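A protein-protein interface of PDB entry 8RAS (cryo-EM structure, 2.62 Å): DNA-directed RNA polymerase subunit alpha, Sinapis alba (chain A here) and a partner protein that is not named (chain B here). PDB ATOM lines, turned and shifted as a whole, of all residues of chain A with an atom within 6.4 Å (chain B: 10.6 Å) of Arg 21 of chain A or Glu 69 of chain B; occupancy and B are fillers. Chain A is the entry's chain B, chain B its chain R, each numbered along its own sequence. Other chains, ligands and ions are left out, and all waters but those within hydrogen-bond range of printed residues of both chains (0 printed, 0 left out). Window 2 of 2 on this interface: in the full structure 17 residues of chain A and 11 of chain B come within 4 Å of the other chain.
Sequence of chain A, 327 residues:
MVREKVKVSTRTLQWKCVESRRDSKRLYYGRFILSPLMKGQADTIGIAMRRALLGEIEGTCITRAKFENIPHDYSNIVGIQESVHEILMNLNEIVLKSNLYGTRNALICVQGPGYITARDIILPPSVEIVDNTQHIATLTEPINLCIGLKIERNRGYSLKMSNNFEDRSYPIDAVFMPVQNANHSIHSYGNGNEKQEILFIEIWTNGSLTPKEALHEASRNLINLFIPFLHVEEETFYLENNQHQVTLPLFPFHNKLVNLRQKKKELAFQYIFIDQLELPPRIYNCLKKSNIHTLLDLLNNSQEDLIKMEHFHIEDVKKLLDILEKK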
ATOM      1  N   GLU A  19     -22.270  -5.804 -21.254  1.00  0.00           N
ATOM      2  CA  GLU A  19     -23.442  -5.609 -22.094  1.00  0.00           C
ATOM      3  C   GLU A  19     -24.676  -5.556 -21.209  1.00  0.00           C
ATOM      4  O   GLU A  19     -24.763  -6.257 -20.198  1.00  0.00           O
ATOM      5  CB  GLU A  19     -23.579  -6.722 -23.138  1.00  0.00           C
ATOM      6  CG  GLU A  19     -24.563  -6.411 -24.251  1.00  0.00           C
ATOM      7  CD  GLU A  19     -24.646  -7.518 -25.283  1.00  0.00           C
ATOM      8  OE1 GLU A  19     -23.692  -8.319 -25.377  1.00  0.00           O
ATOM      9  OE2 GLU A  19     -25.665  -7.587 -26.004  1.00  0.00           O
ATOM     10  N   SER A  20     -25.629  -4.715 -21.602  1.00  0.00           N
ATOM     11  CA  SER A  20     -26.881  -4.570 -20.876  1.00  0.00           C
ATOM     12  C   SER A  20     -27.959  -4.119 -21.848  1.00  0.00           C
ATOM     13  O   SER A  20     -27.689  -3.338 -22.763  1.00  0.00           O
ATOM     14  CB  SER A  20     -26.748  -3.571 -19.723  1.00  0.00           C
ATOM     15  OG  SER A  20     -27.857  -3.655 -18.850  1.00  0.00           O
ATOM     16  N   ARG A  21     -29.178  -4.612 -21.642  1.00  0.00           N
ATOM     17  CA  ARG A  21     -30.286  -4.283 -22.526  1.00  0.00           C
ATOM     18  C   ARG A  21     -31.595  -4.427 -21.767  1.00  0.00           C
ATOM     19  O   ARG A  21     -31.673  -5.117 -20.748  1.00  0.00           O
ATOM     20  CB  ARG A  21     -30.295  -5.175 -23.771  1.00  0.00           C
ATOM     21  CG  ARG A  21     -29.622  -4.562 -24.988  1.00  0.00           C
ATOM     22  CD  ARG A  21     -30.201  -5.117 -26.282  1.00  0.00           C
ATOM     23  NE  ARG A  21     -30.977  -6.330 -26.061  1.00  0.00           N
ATOM     24  CZ  ARG A  21     -30.486  -7.560 -26.144  1.00  0.00           C
ATOM     25  NH1 ARG A  21     -29.216  -7.776 -26.441  1.00  0.00           N
ATOM     26  NH2 ARG A  21     -31.289  -8.595 -25.918  1.00  0.00           N
ATOM     27  N   ARG A  22     -32.626  -3.757 -22.284  1.00  0.00           N
ATOM     28  CA  ARG A  22     -33.994  -3.863 -21.768  1.00  0.00           C
ATOM     29  C   ARG A  22     -34.919  -3.907 -22.983  1.00  0.00           C
ATOM     30  O   ARG A  22     -35.372  -2.868 -23.467  1.00  0.00           O
ATOM     31  CB  ARG A  22     -34.337  -2.703 -20.843  1.00  0.00           C
ATOM     32  CG  ARG A  22     -33.985  -2.934 -19.388  1.00  0.00           C
ATOM     33  CD  ARG A  22     -32.752  -2.139 -18.993  1.00  0.00           C
ATOM     34  NE  ARG A  22     -32.498  -2.192 -17.558  1.00  0.00           N
ATOM     35  CZ  ARG A  22     -31.598  -2.978 -16.984  1.00  0.00           C
ATOM     36  NH1 ARG A  22     -30.844  -3.801 -17.693  1.00  0.00           N
ATOM     37  NH2 ARG A  22     -31.452  -2.937 -15.662  1.00  0.00           N
ATOM     38  N   ASP A  23     -35.194  -5.119 -23.471  1.00  0.00           N
ATOM     39  CA  ASP A  23     -36.064  -5.262 -24.633  1.00  0.00           C
ATOM     40  C   ASP A  23     -37.479  -4.794 -24.323  1.00  0.00           C
ATOM     41  O   ASP A  23     -38.105  -4.099 -25.132  1.00  0.00           O
ATOM     42  CB  ASP A  23     -36.065  -6.713 -25.109  1.00  0.00           C
ATOM     43  CG  ASP A  23     -34.695  -7.176 -25.556  1.00  0.00           C
ATOM     44  OD1 ASP A  23     -34.001  -6.399 -26.246  1.00  0.00           O
ATOM     45  OD2 ASP A  23     -34.308  -8.313 -25.215  1.00  0.00           O
ATOM     46  N   LEU A  27     -38.269  -8.175 -19.829  1.00  0.00           N
ATOM     47  CA  LEU A  27     -37.181  -8.891 -20.493  1.00  0.00           C
ATOM     48  C   LEU A  27     -35.920  -8.045 -20.349  1.00  0.00           C
ATOM     49  O   LEU A  27     -35.733  -7.078 -21.091  1.00  0.00           O
ATOM     50  CB  LEU A  27     -37.499  -9.169 -21.957  1.00  0.00           C
ATOM     51  CG  LEU A  27     -38.506 -10.273 -22.283  1.00  0.00           C
ATOM     52  CD1 LEU A  27     -39.578  -9.768 -23.235  1.00  0.00           C
ATOM     53  CD2 LEU A  27     -37.797 -11.486 -22.861  1.00  0.00           C
ATOM     54  N   TYR A  28     -35.069  -8.413 -19.395  1.00  0.00           N
ATOM     55  CA  TYR A  28     -33.798  -7.746 -19.161  1.00  0.00           C
ATOM     56  C   TYR A  28     -32.662  -8.709 -19.472  1.00  0.00           C
ATOM     57  O   TYR A  28     -32.746  -9.900 -19.162  1.00  0.00           O
ATOM     58  CB  TYR A  28     -33.676  -7.255 -17.714  1.00  0.00           C
ATOM     59  CG  TYR A  28     -34.535  -6.060 -17.349  1.00  0.00           C
ATOM     60  CD1 TYR A  28     -35.777  -5.856 -17.935  1.00  0.00           C
ATOM     61  CD2 TYR A  28     -34.104  -5.142 -16.401  1.00  0.00           C
ATOM     62  CE1 TYR A  28     -36.559  -4.769 -17.599  1.00  0.00           C
ATOM     63  CE2 TYR A  28     -34.880  -4.052 -16.058  1.00  0.00           C
ATOM     64  CZ  TYR A  28     -36.107  -3.871 -16.660  1.00  0.00           C
ATOM     65  OH  TYR A  28     -36.888  -2.789 -16.323  1.00  0.00           O
ATOM     66  N   TYR A  29     -31.602  -8.193 -20.082  1.00  0.00           N
ATOM     67  CA  TYR A  29     -30.436  -8.993 -20.422  1.00  0.00           C
ATOM     68  C   TYR A  29     -29.175  -8.283 -19.953  1.00  0.00           C
ATOM     69  O   TYR A  29     -29.100  -7.052 -19.954  1.00  0.00           O
ATOM     70  CB  TYR A  29     -30.357  -9.264 -21.931  1.00  0.00           C
ATOM     71  CG  TYR A  29     -29.029  -9.820 -22.389  1.00  0.00           C
ATOM     72  CD1 TYR A  29     -28.721 -11.161 -22.220  1.00  0.00           C
ATOM     73  CD2 TYR A  29     -28.082  -9.002 -22.989  1.00  0.00           C
ATOM     74  CE1 TYR A  29     -27.511 -11.673 -22.635  1.00  0.00           C
ATOM     75  CE2 TYR A  29     -26.868  -9.505 -23.404  1.00  0.00           C
ATOM     76  CZ  TYR A  29     -26.589 -10.840 -23.226  1.00  0.00           C
ATOM     77  OH  TYR A  29     -25.381 -11.345 -23.642  1.00  0.00           O
ATOM     78  N   GLY A  30     -28.191  -9.072 -19.552  1.00  0.00           N
ATOM     79  CA  GLY A  30     -26.907  -8.529 -19.145  1.00  0.00           C
ATOM     80  C   GLY A  30     -25.814  -9.551 -19.337  1.00  0.00           C
ATOM     81  O   GLY A  30     -26.037 -10.758 -19.209  1.00  0.00           O
ATOM     82  N   GLU A 202     -24.002 -14.746 -18.698  1.00  0.00           N
ATOM     83  CA  GLU A 202     -25.179 -14.123 -19.286  1.00  0.00           C
ATOM     84  C   GLU A 202     -26.378 -14.391 -18.392  1.00  0.00           C
ATOM     85  O   GLU A 202     -26.589 -15.527 -17.960  1.00  0.00           O
ATOM     86  CB  GLU A 202     -25.447 -14.665 -20.687  1.00  0.00           C
ATOM     87  CG  GLU A 202     -24.648 -14.005 -21.780  1.00  0.00           C
ATOM     88  CD  GLU A 202     -24.854 -14.680 -23.115  1.00  0.00           C
ATOM     89  OE1 GLU A 202     -24.989 -15.920 -23.134  1.00  0.00           O
ATOM     90  OE2 GLU A 202     -24.890 -13.971 -24.141  1.00  0.00           O
ATOM     91  N   TRP A 204     -30.621 -13.552 -18.020  1.00  0.00           N
ATOM     92  CA  TRP A 204     -31.897 -13.035 -18.498  1.00  0.00           C
ATOM     93  C   TRP A 204     -32.876 -13.034 -17.332  1.00  0.00           C
ATOM     94  O   TRP A 204     -33.107 -14.078 -16.715  1.00  0.00           O
ATOM     95  CB  TRP A 204     -32.448 -13.877 -19.648  1.00  0.00           C
ATOM     96  CG  TRP A 204     -31.666 -13.815 -20.924  1.00  0.00           C
ATOM     97  CD1 TRP A 204     -31.915 -13.011 -21.995  1.00  0.00           C
ATOM     98  CD2 TRP A 204     -30.530 -14.612 -21.278  1.00  0.00           C
ATOM     99  NE1 TRP A 204     -30.998 -13.245 -22.988  1.00  0.00           N
ATOM    100  CE2 TRP A 204     -30.135 -14.223 -22.572  1.00  0.00           C
ATOM    101  CE3 TRP A 204     -29.801 -15.607 -20.622  1.00  0.00           C
ATOM    102  CZ2 TRP A 204     -29.047 -14.797 -23.223  1.00  0.00           C
ATOM    103  CZ3 TRP A 204     -28.723 -16.175 -21.270  1.00  0.00           C
ATOM    104  CH2 TRP A 204     -28.356 -15.768 -22.556  1.00  0.00           C
ATOM    105  N   PRO A 211     -30.023  -7.853 -14.067  1.00  0.00           N
ATOM    106  CA  PRO A 211     -28.954  -8.862 -14.138  1.00  0.00           C
ATOM    107  C   PRO A 211     -27.805  -8.603 -13.180  1.00  0.00           C
ATOM    108  O   PRO A 211     -27.225  -9.561 -12.654  1.00  0.00           O
ATOM    109  CB  PRO A 211     -28.505  -8.781 -15.603  1.00  0.00           C
ATOM    110  CG  PRO A 211     -29.722  -8.331 -16.328  1.00  0.00           C
ATOM    111  CD  PRO A 211     -30.412  -7.370 -15.403  1.00  0.00           C
ATOM    112  N   PRO B  66     -36.199 -14.638 -27.866  1.00  0.00           N
ATOM    113  CA  PRO B  66     -35.554 -13.430 -27.342  1.00  0.00           C
ATOM    114  C   PRO B  66     -34.319 -13.740 -26.501  1.00  0.00           C
ATOM    115  O   PRO B  66     -33.808 -12.858 -25.811  1.00  0.00           O
ATOM    116  CB  PRO B  66     -36.650 -12.786 -26.484  1.00  0.00           C
ATOM    117  CG  PRO B  66     -37.637 -13.880 -26.224  1.00  0.00           C
ATOM    118  CD  PRO B  66     -37.607 -14.730 -27.447  1.00  0.00           C
ATOM    119  N   PHE B  67     -33.847 -14.980 -26.566  1.00  0.00           N
ATOM    120  CA  PHE B  67     -32.662 -15.423 -25.844  1.00  0.00           C
ATOM    121  C   PHE B  67     -31.571 -15.853 -26.815  1.00  0.00           C
ATOM    122  O   PHE B  67     -30.878 -16.849 -26.603  1.00  0.00           O
ATOM    123  CB  PHE B  67     -32.998 -16.560 -24.881  1.00  0.00           C
ATOM    124  CG  PHE B  67     -34.117 -16.243 -23.931  1.00  0.00           C
ATOM    125  CD1 PHE B  67     -35.433 -16.488 -24.281  1.00  0.00           C
ATOM    126  CD2 PHE B  67     -33.852 -15.704 -22.685  1.00  0.00           C
ATOM    127  CE1 PHE B  67     -36.462 -16.198 -23.408  1.00  0.00           C
ATOM    128  CE2 PHE B  67     -34.875 -15.413 -21.809  1.00  0.00           C
ATOM    129  CZ  PHE B  67     -36.182 -15.660 -22.170  1.00  0.00           C
ATOM    130  N   VAL B  68     -31.407 -15.100 -27.899  1.00  0.00           N
ATOM    131  CA  VAL B  68     -30.472 -15.448 -28.959  1.00  0.00           C
ATOM    132  C   VAL B  68     -29.275 -14.499 -28.983  1.00  0.00           C
ATOM    133  O   VAL B  68     -28.566 -14.428 -29.984  1.00  0.00           O
ATOM    134  CB  VAL B  68     -31.177 -15.490 -30.325  1.00  0.00           C
ATOM    135  CG1 VAL B  68     -32.192 -16.616 -30.359  1.00  0.00           C
ATOM    136  CG2 VAL B  68     -31.847 -14.159 -30.612  1.00  0.00           C
ATOM    137  N   GLU B  69     -29.043 -13.764 -27.894  1.00  0.00           N
ATOM    138  CA  GLU B  69     -27.921 -12.832 -27.852  1.00  0.00           C
ATOM    139  C   GLU B  69     -26.593 -13.564 -28.005  1.00  0.00           C
ATOM    140  O   GLU B  69     -25.742 -13.171 -28.812  1.00  0.00           O
ATOM    141  CB  GLU B  69     -27.951 -12.039 -26.546  1.00  0.00           C
ATOM    142  CG  GLU B  69     -29.116 -11.077 -26.431  1.00  0.00           C
ATOM    143  CD  GLU B  69     -30.357 -11.732 -25.865  1.00  0.00           C
ATOM    144  OE1 GLU B  69     -30.295 -12.932 -25.529  1.00  0.00           O
ATOM    145  OE2 GLU B  69     -31.396 -11.050 -25.756  1.00  0.00           O
ATOM    146  N   GLU B  70     -26.408 -14.644 -27.243  1.00  0.00           N
ATOM    147  CA  GLU B  70     -25.200 -15.448 -27.385  1.00  0.00           C
ATOM    148  C   GLU B  70     -25.117 -16.058 -28.775  1.00  0.00           C
ATOM    149  O   GLU B  70     -24.036 -16.126 -29.368  1.00  0.00           O
ATOM    150  CB  GLU B  70     -25.165 -16.541 -26.316  1.00  0.00           C
ATOM    151  CG  GLU B  70     -24.008 -17.526 -26.451  1.00  0.00           C
ATOM    152  CD  GLU B  70     -22.642 -16.861 -26.385  1.00  0.00           C
ATOM    153  OE1 GLU B  70     -22.500 -15.848 -25.671  1.00  0.00           O
ATOM    154  OE2 GLU B  70     -21.707 -17.357 -27.048  1.00  0.00           O
ATOM    155  N   GLN B  71     -26.255 -16.493 -29.313  1.00  0.00           N
ATOM    156  CA  GLN B  71     -26.279 -17.097 -30.640  1.00  0.00           C
ATOM    157  C   GLN B  71     -25.876 -16.093 -31.714  1.00  0.00           C
ATOM    158  O   GLN B  71     -25.034 -16.390 -32.570  1.00  0.00           O
ATOM    159  CB  GLN B  71     -27.671 -17.653 -30.916  1.00  0.00           C
ATOM    160  CG  GLN B  71     -27.681 -18.962 -31.658  1.00  0.00           C
ATOM    161  CD  GLN B  71     -29.057 -19.316 -32.151  1.00  0.00           C
ATOM    162  OE1 GLN B  71     -30.048 -19.144 -31.443  1.00  0.00           O
ATOM    163  NE2 GLN B  71     -29.132 -19.811 -33.372  1.00  0.00           N
ATOM    164  N   VAL B  72     -26.467 -14.897 -31.683  1.00  0.00           N
ATOM    165  CA  VAL B  72     -26.136 -13.869 -32.666  1.00  0.00           C
ATOM    166  C   VAL B  72     -24.676 -13.458 -32.537  1.00  0.00           C
ATOM    167  O   VAL B  72     -23.966 -13.300 -33.541  1.00  0.00           O
ATOM    168  CB  VAL B  72     -27.081 -12.662 -32.508  1.00  0.00           C
ATOM    169  CG1 VAL B  72     -26.553 -11.466 -33.282  1.00  0.00           C
ATOM    170  CG2 VAL B  72     -28.482 -13.021 -32.967  1.00  0.00           C
ATOM    171  N   ARG B  73     -24.204 -13.276 -31.302  1.00  0.00           N
ATOM    172  CA  ARG B  73     -22.814 -12.890 -31.098  1.00  0.00           C
ATOM    173  C   ARG B  73     -21.861 -13.962 -31.611  1.00  0.00           C
ATOM    174  O   ARG B  73     -20.848 -13.648 -32.241  1.00  0.00           O
ATOM    175  CB  ARG B  73     -22.563 -12.606 -29.620  1.00  0.00           C
ATOM    176  CG  ARG B  73     -21.158 -12.133 -29.313  1.00  0.00           C
ATOM    177  CD  ARG B  73     -21.010 -11.802 -27.844  1.00  0.00           C
ATOM    178  NE  ARG B  73     -21.586 -12.838 -26.997  1.00  0.00           N
ATOM    179  CZ  ARG B  73     -22.657 -12.670 -26.234  1.00  0.00           C
ATOM    180  NH1 ARG B  73     -23.307 -11.519 -26.197  1.00  0.00           N
ATOM    181  NH2 ARG B  73     -23.087 -13.684 -25.491  1.00  0.00           N
ATOM    182  N   LYS B  74     -22.175 -15.233 -31.359  1.00  0.00           N
ATOM    183  CA  LYS B  74     -21.328 -16.317 -31.839  1.00  0.00           C
ATOM    184  C   LYS B  74     -21.341 -16.386 -33.362  1.00  0.00           C
ATOM    185  O   LYS B  74     -20.304 -16.644 -33.986  1.00  0.00           O
ATOM    186  CB  LYS B  74     -21.790 -17.641 -31.224  1.00  0.00           C
ATOM    187  CG  LYS B  74     -21.167 -18.900 -31.815  1.00  0.00           C
ATOM    188  CD  LYS B  74     -19.643 -18.867 -31.787  1.00  0.00           C
ATOM    189  CE  LYS B  74     -19.102 -18.624 -30.384  1.00  0.00           C
ATOM    190  NZ  LYS B  74     -17.834 -17.844 -30.403  1.00  0.00           N
ATOM    191  N   ILE B  75     -22.504 -16.152 -33.976  1.00  0.00           N
ATOM    192  CA  ILE B  75     -22.591 -16.129 -35.435  1.00  0.00           C
ATOM    193  C   ILE B  75     -21.688 -15.040 -35.996  1.00  0.00           C
ATOM    194  O   ILE B  75     -20.948 -15.254 -36.962  1.00  0.00           O
ATOM    195  CB  ILE B  75     -24.048 -15.931 -35.887  1.00  0.00           C
ATOM    196  CG1 ILE B  75     -24.863 -17.203 -35.671  1.00  0.00           C
ATOM    197  CG2 ILE B  75     -24.104 -15.530 -37.349  1.00  0.00           C
ATOM    198  CD1 ILE B  75     -26.330 -17.027 -35.972  1.00  0.00           C
ATOM    199  N   LYS B  76     -21.734 -13.852 -35.390  1.00  0.00           N
ATOM    200  CA  LYS B  76     -20.872 -12.766 -35.843  1.00  0.00           C
ATOM    201  C   LYS B  76     -19.399 -13.100 -35.630  1.00  0.00           C
ATOM    202  O   LYS B  76     -18.555 -12.780 -36.476  1.00  0.00           O
ATOM    203  CB  LYS B  76     -21.242 -11.468 -35.127  1.00  0.00           C
ATOM    204  CG  LYS B  76     -22.326 -10.674 -35.831  1.00  0.00           C
ATOM    205  CD  LYS B  76     -23.415 -10.241 -34.867  1.00  0.00           C
ATOM    206  CE  LYS B  76     -24.417  -9.326 -35.548  1.00  0.00           C
ATOM    207  NZ  LYS B  76     -23.891  -7.941 -35.696  1.00  0.00           N
ATOM    208  N   GLU B  77     -19.070 -13.741 -34.506  1.00  0.00           N
ATOM    209  CA  GLU B  77     -17.678 -14.075 -34.220  1.00  0.00           C
ATOM    210  C   GLU B  77     -17.119 -15.082 -35.218  1.00  0.00           C
ATOM    211  O   GLU B  77     -15.979 -14.940 -35.674  1.00  0.00           O
ATOM    212  CB  GLU B  77     -17.542 -14.612 -32.796  1.00  0.00           C
ATOM    213  CG  GLU B  77     -17.799 -13.584 -31.709  1.00  0.00           C
ATOM    214  CD  GLU B  77     -17.831 -14.202 -30.325  1.00  0.00           C
ATOM    215  OE1 GLU B  77     -17.508 -15.403 -30.202  1.00  0.00           O
ATOM    216  OE2 GLU B  77     -18.180 -13.491 -29.360  1.00  0.00           O
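NE1 of Trp 204 of chain A sits at hydrogen-bond distance from OE1 of Glu 69 of chain B (2.7 Å).
The side-chain hydroxyl (OH) of Tyr 29 of chain A lies within hydrogen-bond range of the guanidinium group (NH1) of Arg 73 of chain B, 3.3 Å away.
OE2 of Glu 202 of chain A sits close to OE1 of Glu 70 of chain B (3.4 Å).
The side-chain carboxylate (OE1) of Glu 19 of chain A lies within salt-bridge range of the guanidinium group (NH1) of Arg 73 of chain B.
The guanidinium group (NH1) of Arg 73 of chain B lies within salt-bridge range of the side-chain carboxylate (OE2) of Glu 202 of chain A, at 3.6 Å.
The guanidinium group (NH2) of Arg 21 of chain A lies within salt-bridge range of the side-chain carboxylate (OE2) of Glu 69 of chain B (2.5 Å).
NH1 of Arg 21 of chain A lies within salt-bridge range of OE2 of Glu 19 of chain A (3.6 Å).
The guanidinium group (NE) of Arg 21 of chain A is in salt-bridge range of the side-chain carboxylate (OD1) of Asp 23 of chain A.
N of Arg 21 of chain A is in hydrogen-bond range of O of Tyr 29 of chain A (3.0 Å).
OE1 of Glu 70 of chain B is in salt-bridge range of NE of Arg 73 of chain B.
OH of Tyr 29 of chain A is in hydrogen-bond range of OE2 of Glu 202 of chain A (2.7 Å).
Tyr 29 of chain A touches Glu 69 of chain B.
CG of Trp 204 of chain A touches CD2 of Phe 67 of chain B, 3.4 Å away.
No residue of chain B comes within 4 Å of Ser 20 of chain A.
Arg 21 of chain A touches just one residue of chain B: Glu 69 (2.5 Å).
No residue of chain B comes within 4 Å of Arg 22 of chain A.
Of chain B, only Glu 69 and Arg 73 come within 4 Å of Tyr 29 of chain A.
Printed residues of chain B within 4 Å of Glu 202 of chain A: Glu 70 and Arg 73.
Printed residues of chain B within 4 Å of Trp 204 of chain A: Phe 67 and Glu 69.
Of chain A, only Arg 21, Tyr 29 and Trp 204 come within 4 Å of Glu 69 of chain B.
Printed residues of chain A within 4 Å of Glu 70 of chain B: Glu 202 (3.2 Å).
Printed residues of chain A that touch a printed residue of chain B: Glu 19, Arg 21, Tyr 29, Glu 202 and Trp 204.
Hydrophobic or aromatic side chains of chain A within 4 Å of the printed part of chain B: Tyr 29 and Trp 204.
Of the 12 printed residues of chain B, 4 touch a printed residue of chain A.
Hydrophobic or aromatic side chains of chain B within 4 Å of the printed part of chain A: Phe 67.
Among the printed residues, Asp or Glu carboxylates within 4 Å of a Lys or Arg side-chain nitrogen of the other chain: Glu 19 of chain A with Arg 73 of chain B, Arg 21 of chain A with Glu 69 of chain B and Glu 202 of chain A with Arg 73 of chain B.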
